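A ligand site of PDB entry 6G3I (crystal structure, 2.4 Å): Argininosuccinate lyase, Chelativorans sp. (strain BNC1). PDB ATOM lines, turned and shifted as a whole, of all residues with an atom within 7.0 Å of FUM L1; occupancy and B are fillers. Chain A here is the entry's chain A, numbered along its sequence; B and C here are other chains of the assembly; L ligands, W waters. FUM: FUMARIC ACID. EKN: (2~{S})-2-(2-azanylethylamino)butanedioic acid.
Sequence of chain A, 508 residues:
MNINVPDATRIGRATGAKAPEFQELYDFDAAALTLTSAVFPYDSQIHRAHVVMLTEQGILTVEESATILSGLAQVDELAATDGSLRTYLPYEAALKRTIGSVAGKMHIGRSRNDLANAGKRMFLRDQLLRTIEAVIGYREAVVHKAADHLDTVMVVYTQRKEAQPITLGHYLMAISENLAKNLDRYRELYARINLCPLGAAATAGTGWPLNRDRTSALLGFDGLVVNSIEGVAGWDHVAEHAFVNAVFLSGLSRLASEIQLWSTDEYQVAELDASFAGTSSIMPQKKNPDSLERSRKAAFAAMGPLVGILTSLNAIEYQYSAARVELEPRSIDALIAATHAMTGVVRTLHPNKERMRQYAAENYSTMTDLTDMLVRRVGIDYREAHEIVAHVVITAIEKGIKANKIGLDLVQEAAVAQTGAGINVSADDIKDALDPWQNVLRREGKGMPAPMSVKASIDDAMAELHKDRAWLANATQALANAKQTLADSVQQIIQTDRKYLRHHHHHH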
ATOM      1  N   THR A   9      31.197  27.676 -13.919  1.00  0.00           N
ATOM      2  CA  THR A   9      30.156  28.597 -13.498  1.00  0.00           C
ATOM      3  C   THR A   9      30.669  29.671 -12.550  1.00  0.00           C
ATOM      4  O   THR A   9      29.967  30.669 -12.324  1.00  0.00           O
ATOM      5  CB  THR A   9      29.017  27.843 -12.808  1.00  0.00           C
ATOM      6  OG1 THR A   9      29.460  27.324 -11.539  1.00  0.00           O
ATOM      7  CG2 THR A   9      28.525  26.695 -13.672  1.00  0.00           C
ATOM      8  N   LYS A  18      32.031  26.931  -5.298  1.00  0.00           N
ATOM      9  CA  LYS A  18      30.815  26.522  -4.616  1.00  0.00           C
ATOM     10  C   LYS A  18      31.173  25.922  -3.269  1.00  0.00           C
ATOM     11  O   LYS A  18      32.102  25.116  -3.171  1.00  0.00           O
ATOM     12  CB  LYS A  18      30.043  25.485  -5.437  1.00  0.00           C
ATOM     13  CG  LYS A  18      29.563  25.922  -6.811  1.00  0.00           C
ATOM     14  CD  LYS A  18      28.319  25.116  -7.206  1.00  0.00           C
ATOM     15  CE  LYS A  18      28.156  24.993  -8.703  1.00  0.00           C
ATOM     16  NZ  LYS A  18      29.029  23.935  -9.282  1.00  0.00           N
ATOM     17  N   PHE A  22      26.590  23.525  -1.083  1.00  0.00           N
ATOM     18  CA  PHE A  22      25.951  24.037  -2.283  1.00  0.00           C
ATOM     19  C   PHE A  22      26.145  23.077  -3.459  1.00  0.00           C
ATOM     20  O   PHE A  22      25.234  22.873  -4.266  1.00  0.00           O
ATOM     21  CB  PHE A  22      26.527  25.423  -2.601  1.00  0.00           C
ATOM     22  CG  PHE A  22      25.918  26.107  -3.791  1.00  0.00           C
ATOM     23  CD1 PHE A  22      24.669  25.756  -4.281  1.00  0.00           C
ATOM     24  CD2 PHE A  22      26.607  27.124  -4.422  1.00  0.00           C
ATOM     25  CE1 PHE A  22      24.130  26.399  -5.382  1.00  0.00           C
ATOM     26  CE2 PHE A  22      26.081  27.772  -5.525  1.00  0.00           C
ATOM     27  CZ  PHE A  22      24.842  27.404  -6.001  1.00  0.00           C
ATOM     28  N   TYR A  26      23.871  19.838  -6.827  1.00  0.00           N
ATOM     29  CA  TYR A  26      24.132  19.535  -8.230  1.00  0.00           C
ATOM     30  C   TYR A  26      24.516  18.073  -8.460  1.00  0.00           C
ATOM     31  O   TYR A  26      24.494  17.617  -9.614  1.00  0.00           O
ATOM     32  CB  TYR A  26      25.241  20.438  -8.762  1.00  0.00           C
ATOM     33  CG  TYR A  26      24.824  21.885  -8.866  1.00  0.00           C
ATOM     34  CD1 TYR A  26      24.817  22.712  -7.747  1.00  0.00           C
ATOM     35  CD2 TYR A  26      24.420  22.424 -10.078  1.00  0.00           C
ATOM     36  CE1 TYR A  26      24.430  24.022  -7.837  1.00  0.00           C
ATOM     37  CE2 TYR A  26      24.025  23.749 -10.173  1.00  0.00           C
ATOM     38  CZ  TYR A  26      24.030  24.549  -9.052  1.00  0.00           C
ATOM     39  OH  TYR A  26      23.645  25.857  -9.133  1.00  0.00           O
ATOM     40  N   GLY A 278      25.351  32.053  -7.315  1.00  0.00           N
ATOM     41  CA  GLY A 278      25.901  31.954  -8.650  1.00  0.00           C
ATOM     42  C   GLY A 278      25.732  33.251  -9.401  1.00  0.00           C
ATOM     43  O   GLY A 278      25.506  34.298  -8.778  1.00  0.00           O
ATOM     44  N   THR A 279      25.833  33.210 -10.725  1.00  0.00           N
ATOM     45  CA  THR A 279      25.627  34.408 -11.531  1.00  0.00           C
ATOM     46  C   THR A 279      25.125  33.994 -12.903  1.00  0.00           C
ATOM     47  O   THR A 279      24.922  32.804 -13.185  1.00  0.00           O
ATOM     48  CB  THR A 279      26.922  35.234 -11.632  1.00  0.00           C
ATOM     49  OG1 THR A 279      26.669  36.437 -12.382  1.00  0.00           O
ATOM     50  CG2 THR A 279      28.028  34.435 -12.306  1.00  0.00           C
ATOM     51  N   ASP A 290      20.895  30.526  -6.315  1.00  0.00           N
ATOM     52  CA  ASP A 290      20.766  29.164  -6.834  1.00  0.00           C
ATOM     53  C   ASP A 290      20.635  28.149  -5.711  1.00  0.00           C
ATOM     54  O   ASP A 290      19.875  27.182  -5.832  1.00  0.00           O
ATOM     55  CB  ASP A 290      21.969  28.829  -7.714  1.00  0.00           C
ATOM     56  CG  ASP A 290      22.045  29.684  -8.965  1.00  0.00           C
ATOM     57  OD1 ASP A 290      20.989  30.188  -9.396  1.00  0.00           O
ATOM     58  OD2 ASP A 290      23.151  29.852  -9.515  1.00  0.00           O
ATOM     59  N   SER A 291      21.357  28.361  -4.610  1.00  0.00           N
ATOM     60  CA  SER A 291      21.236  27.460  -3.464  1.00  0.00           C
ATOM     61  C   SER A 291      19.811  27.451  -2.944  1.00  0.00           C
ATOM     62  O   SER A 291      19.240  26.388  -2.670  1.00  0.00           O
ATOM     63  CB  SER A 291      22.215  27.888  -2.369  1.00  0.00           C
ATOM     64  OG  SER A 291      22.043  29.252  -2.036  1.00  0.00           O
ATOM     65  N   GLU A 293      16.901  28.408  -4.468  1.00  0.00           N
ATOM     66  CA  GLU A 293      15.857  27.979  -5.388  1.00  0.00           C
ATOM     67  C   GLU A 293      15.935  26.474  -5.665  1.00  0.00           C
ATOM     68  O   GLU A 293      14.899  25.840  -5.862  1.00  0.00           O
ATOM     69  CB  GLU A 293      15.951  28.756  -6.694  1.00  0.00           C
ATOM     70  CG  GLU A 293      15.493  30.206  -6.565  1.00  0.00           C
ATOM     71  CD  GLU A 293      15.211  30.868  -7.896  1.00  0.00           C
ATOM     72  OE1 GLU A 293      14.522  31.898  -7.898  1.00  0.00           O
ATOM     73  OE2 GLU A 293      15.669  30.347  -8.934  1.00  0.00           O
ATOM     74  N   ARG A 294      17.136  25.900  -5.679  1.00  0.00           N
ATOM     75  CA  ARG A 294      17.247  24.455  -5.834  1.00  0.00           C
ATOM     76  C   ARG A 294      16.856  23.727  -4.558  1.00  0.00           C
ATOM     77  O   ARG A 294      16.411  22.568  -4.624  1.00  0.00           O
ATOM     78  CB  ARG A 294      18.658  24.074  -6.259  1.00  0.00           C
ATOM     79  CG  ARG A 294      18.877  24.143  -7.768  1.00  0.00           C
ATOM     80  CD  ARG A 294      20.315  23.878  -8.153  1.00  0.00           C
ATOM     81  NE  ARG A 294      20.515  23.982  -9.596  1.00  0.00           N
ATOM     82  CZ  ARG A 294      20.467  22.963 -10.449  1.00  0.00           C
ATOM     83  NH1 ARG A 294      20.220  21.737 -10.030  1.00  0.00           N
ATOM     84  NH2 ARG A 294      20.663  23.185 -11.748  1.00  0.00           N
ATOM     85  N   LYS A 297      13.099  23.688  -4.888  1.00  0.00           N
ATOM     86  CA  LYS A 297      12.775  22.678  -5.891  1.00  0.00           C
ATOM     87  C   LYS A 297      12.645  21.309  -5.260  1.00  0.00           C
ATOM     88  O   LYS A 297      11.699  20.564  -5.526  1.00  0.00           O
ATOM     89  CB  LYS A 297      13.848  22.687  -6.965  1.00  0.00           C
ATOM     90  CG  LYS A 297      13.587  21.804  -8.167  1.00  0.00           C
ATOM     91  CD  LYS A 297      14.630  22.069  -9.239  1.00  0.00           C
ATOM     92  CE  LYS A 297      15.159  20.810  -9.881  1.00  0.00           C
ATOM     93  NZ  LYS A 297      16.509  21.048 -10.467  1.00  0.00           N
ATOM     94  N   THR B  87      26.491  20.415 -19.430  1.00  0.00           N
ATOM     95  CA  THR B  87      25.808  21.643 -19.062  1.00  0.00           C
ATOM     96  C   THR B  87      26.520  22.800 -19.763  1.00  0.00           C
ATOM     97  O   THR B  87      27.683  22.684 -20.170  1.00  0.00           O
ATOM     98  CB  THR B  87      25.775  21.853 -17.548  1.00  0.00           C
ATOM     99  OG1 THR B  87      27.100  22.037 -17.062  1.00  0.00           O
ATOM    100  CG2 THR B  87      25.156  20.633 -16.864  1.00  0.00           C
ATOM    101  N   TYR B  88      25.807  23.922 -19.907  1.00  0.00           N
ATOM    102  CA  TYR B  88      26.207  24.891 -20.920  1.00  0.00           C
ATOM    103  C   TYR B  88      27.621  25.417 -20.685  1.00  0.00           C
ATOM    104  O   TYR B  88      28.489  25.309 -21.554  1.00  0.00           O
ATOM    105  CB  TYR B  88      25.231  26.067 -20.975  1.00  0.00           C
ATOM    106  CG  TYR B  88      25.712  27.087 -21.975  1.00  0.00           C
ATOM    107  CD1 TYR B  88      25.800  26.756 -23.320  1.00  0.00           C
ATOM    108  CD2 TYR B  88      26.121  28.347 -21.582  1.00  0.00           C
ATOM    109  CE1 TYR B  88      26.259  27.656 -24.246  1.00  0.00           C
ATOM    110  CE2 TYR B  88      26.587  29.266 -22.506  1.00  0.00           C
ATOM    111  CZ  TYR B  88      26.648  28.913 -23.838  1.00  0.00           C
ATOM    112  OH  TYR B  88      27.112  29.812 -24.777  1.00  0.00           O
ATOM    113  N   SER B 111      20.880  33.293 -23.794  1.00  0.00           N
ATOM    114  CA  SER B 111      21.051  33.035 -22.374  1.00  0.00           C
ATOM    115  C   SER B 111      20.958  31.539 -22.141  1.00  0.00           C
ATOM    116  O   SER B 111      20.522  30.774 -23.007  1.00  0.00           O
ATOM    117  CB  SER B 111      19.983  33.767 -21.545  1.00  0.00           C
ATOM    118  OG  SER B 111      20.055  33.416 -20.174  1.00  0.00           O
ATOM    119  N   ARG B 112      21.387  31.101 -20.944  1.00  0.00           N
ATOM    120  CA  ARG B 112      21.094  29.742 -20.534  1.00  0.00           C
ATOM    121  C   ARG B 112      19.595  29.540 -20.356  1.00  0.00           C
ATOM    122  O   ARG B 112      19.097  28.415 -20.516  1.00  0.00           O
ATOM    123  CB  ARG B 112      21.834  29.417 -19.232  1.00  0.00           C
ATOM    124  CG  ARG B 112      23.265  28.946 -19.429  1.00  0.00           C
ATOM    125  CD  ARG B 112      23.942  28.591 -18.108  1.00  0.00           C
ATOM    126  NE  ARG B 112      23.767  29.627 -17.099  1.00  0.00           N
ATOM    127  CZ  ARG B 112      24.213  29.540 -15.848  1.00  0.00           C
ATOM    128  NH1 ARG B 112      24.874  28.456 -15.438  1.00  0.00           N
ATOM    129  NH2 ARG B 112      24.000  30.534 -14.997  1.00  0.00           N
ATOM    130  N   ASN B 113      18.856  30.614 -20.062  1.00  0.00           N
ATOM    131  CA  ASN B 113      17.446  30.497 -19.729  1.00  0.00           C
ATOM    132  C   ASN B 113      16.620  30.068 -20.937  1.00  0.00           C
ATOM    133  O   ASN B 113      15.827  29.115 -20.845  1.00  0.00           O
ATOM    134  CB  ASN B 113      16.942  31.832 -19.170  1.00  0.00           C
ATOM    135  CG  ASN B 113      17.543  32.136 -17.807  1.00  0.00           C
ATOM    136  OD1 ASN B 113      18.353  31.382 -17.297  1.00  0.00           O
ATOM    137  ND2 ASN B 113      17.144  33.266 -17.227  1.00  0.00           N
ATOM    138  N   ALA B 116      17.833  26.544 -22.247  1.00  0.00           N
ATOM    139  CA  ALA B 116      17.259  25.429 -21.498  1.00  0.00           C
ATOM    140  C   ALA B 116      15.794  25.208 -21.883  1.00  0.00           C
ATOM    141  O   ALA B 116      15.379  24.081 -22.160  1.00  0.00           O
ATOM    142  CB  ALA B 116      17.387  25.689 -20.003  1.00  0.00           C
ATOM    143  N   LYS B 120      14.776  21.673 -23.546  1.00  0.00           N
ATOM    144  CA  LYS B 120      13.853  20.777 -22.849  1.00  0.00           C
ATOM    145  C   LYS B 120      12.568  20.577 -23.655  1.00  0.00           C
ATOM    146  O   LYS B 120      12.013  19.474 -23.680  1.00  0.00           O
ATOM    147  CB  LYS B 120      13.561  21.316 -21.458  1.00  0.00           C
ATOM    148  CG  LYS B 120      14.671  21.044 -20.460  1.00  0.00           C
ATOM    149  CD  LYS B 120      14.718  22.103 -19.365  1.00  0.00           C
ATOM    150  CE  LYS B 120      15.875  21.849 -18.418  1.00  0.00           C
ATOM    151  NZ  LYS B 120      15.938  22.868 -17.326  1.00  0.00           N
ATOM    152  N   TYR B 320      11.459  33.585 -14.934  1.00  0.00           N
ATOM    153  CA  TYR B 320      12.358  32.444 -14.979  1.00  0.00           C
ATOM    154  C   TYR B 320      12.762  32.100 -13.543  1.00  0.00           C
ATOM    155  O   TYR B 320      12.975  32.993 -12.719  1.00  0.00           O
ATOM    156  CB  TYR B 320      13.601  32.748 -15.818  1.00  0.00           C
ATOM    157  CG  TYR B 320      14.653  31.670 -15.665  1.00  0.00           C
ATOM    158  CD1 TYR B 320      14.654  30.560 -16.499  1.00  0.00           C
ATOM    159  CD2 TYR B 320      15.602  31.747 -14.664  1.00  0.00           C
ATOM    160  CE1 TYR B 320      15.603  29.562 -16.344  1.00  0.00           C
ATOM    161  CE2 TYR B 320      16.546  30.761 -14.505  1.00  0.00           C
ATOM    162  CZ  TYR B 320      16.540  29.666 -15.344  1.00  0.00           C
ATOM    163  OH  TYR B 320      17.484  28.681 -15.185  1.00  0.00           O
ATOM    164  N   ALA B 322      14.773  28.757 -11.117  1.00  0.00           N
ATOM    165  CA  ALA B 322      15.416  27.451 -11.017  1.00  0.00           C
ATOM    166  C   ALA B 322      14.739  26.552 -10.003  1.00  0.00           C
ATOM    167  O   ALA B 322      15.221  25.445  -9.753  1.00  0.00           O
ATOM    168  CB  ALA B 322      16.895  27.626 -10.667  1.00  0.00           C
ATOM    169  N   GLN C 159      14.712  34.836 -10.967  1.00  0.00           N
ATOM    170  CA  GLN C 159      15.114  34.341  -9.650  1.00  0.00           C
ATOM    171  C   GLN C 159      14.977  35.408  -8.570  1.00  0.00           C
ATOM    172  O   GLN C 159      15.756  35.445  -7.619  1.00  0.00           O
ATOM    173  CB  GLN C 159      16.549  33.815  -9.670  1.00  0.00           C
ATOM    174  CG  GLN C 159      16.832  32.793 -10.746  1.00  0.00           C
ATOM    175  CD  GLN C 159      18.248  32.242 -10.661  1.00  0.00           C
ATOM    176  OE1 GLN C 159      19.177  32.832 -11.207  1.00  0.00           O
ATOM    177  NE2 GLN C 159      18.411  31.121  -9.974  1.00  0.00           N
HETATM  178  OXT FUM L   1      20.569  26.360 -10.760  1.00  0.00           O
HETATM  179  C   FUM L   1      21.378  26.764 -11.625  1.00  0.00           C
HETATM  180  O   FUM L   1      22.604  26.778 -11.384  1.00  0.00           O
HETATM  181  C4  FUM L   1      20.916  27.235 -12.985  1.00  0.00           C
HETATM  182  C5  FUM L   1      21.496  26.715 -14.033  1.00  0.00           C
HETATM  183  C6  FUM L   1      21.053  27.212 -15.402  1.00  0.00           C
HETATM  184  O7  FUM L   1      20.913  26.424 -16.370  1.00  0.00           O
HETATM  185  O8  FUM L   1      20.837  28.450 -15.531  1.00  0.00           O
HETATM  186  OD1 EKN L   2      22.033  33.165 -18.833  1.00  0.00           O
HETATM  187  CG  EKN L   2      21.865  33.042 -17.540  1.00  0.00           C
HETATM  188  OD2 EKN L   2      22.618  32.376 -16.805  1.00  0.00           O
HETATM  189  CB  EKN L   2      20.744  33.693 -16.863  1.00  0.00           C
HETATM  190  CA  EKN L   2      20.667  33.408 -15.376  1.00  0.00           C
HETATM  191  C   EKN L   2      19.813  34.419 -14.655  1.00  0.00           C
HETATM  192  OXT EKN L   2      20.446  35.089 -13.829  1.00  0.00           O
HETATM  193  O   EKN L   2      18.608  34.505 -14.888  1.00  0.00           O
HETATM  194  N   EKN L   2      20.134  31.983 -15.184  1.00  0.00           N
HETATM  195  CAG EKN L   2      19.975  31.571 -13.715  1.00  0.00           C
HETATM  196  CAF EKN L   2      21.040  30.622 -13.188  1.00  0.00           C
HETATM  197  NAA EKN L   2      22.046  31.403 -12.305  1.00  0.00           N
HETATM  198  O   HOH W   1      20.992  26.218 -19.681  1.00  0.00           O
HETATM  199  O   HOH W   2      25.072  28.178  -9.519  1.00  0.00           O
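The side-chain hydroxyl (OG) of Ser 111 of chain B is in hydrogen-bond range of an oxygen (OD1) of EKN L2, at 2.4 Å.
NE of Arg 294 is in salt-bridge range of OXT of FUM L1, at 2.6 Å.
OH of Tyr 26 sits at hydrogen-bond distance from O of FUM L1 (2.6 Å).
N of Arg 112 of chain B lies within hydrogen-bond range of OD1 of EKN L2 (3.0 Å).
A nitrogen (NAA) of EKN L2 sits at hydrogen-bond distance from the backbone carbonyl oxygen (O) of Thr 279.
O8 of FUM L1 is in salt-bridge range of NE of Arg 112 of chain B (3.5 Å).
A nitrogen (N) of EKN L2 sits at hydrogen-bond distance from the side-chain amide oxygen (OD1) of Asn 113 of chain B (2.8 Å).
The side-chain hydroxyl of Tyr 320 of chain B is in hydrogen-bond range of an oxygen (O8) of FUM L1 (3.4 Å).
The guanidinium group (NH2) of Arg 112 of chain B is in salt-bridge range of an oxygen (OD2) of EKN L2, at 2.9 Å.
The side-chain carboxylate (OD1) of Asp 290 lies within salt-bridge range of a nitrogen (NAA) of EKN L2 (3.3 Å).
OE1 of Gln 159 of chain C sits close to NAA of EKN L2.
The side-chain carboxylate of Asp 290 is in hydrogen-bond range of the side-chain amide nitrogen of Gln 159 of chain C, 2.8 Å away.
The backbone carbonyl oxygen (O) of Thr 279 lies within hydrogen-bond range of the guanidinium group (NH2) of Arg 112 of chain B (3.0 Å).
OE2 of Glu 293 sits at hydrogen-bond distance from N of Ala 322 of chain B (2.8 Å).
O of Tyr 320 of chain B is in hydrogen-bond range of N of Gln 159 of chain C (3.1 Å).
Asp 290 touches FUM L1.
CB of Ala 322 of chain B touches OXT of FUM L1, at 3.9 Å.
Hydrophobic or aromatic side chains that line FUM L1: Tyr 26 and Ala 322 of chain B.
Of the 21 residues printed, 6 come within 4 Å of FUM L1.
Water W1 bridges O of Arg 112 of chain B (3.0 Å) and O7 of FUM L1 (3.3 Å).
Water W2 lies within hydrogen-bond range of OD2 of Asp 290, OH of Tyr 26 and O of FUM L1.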
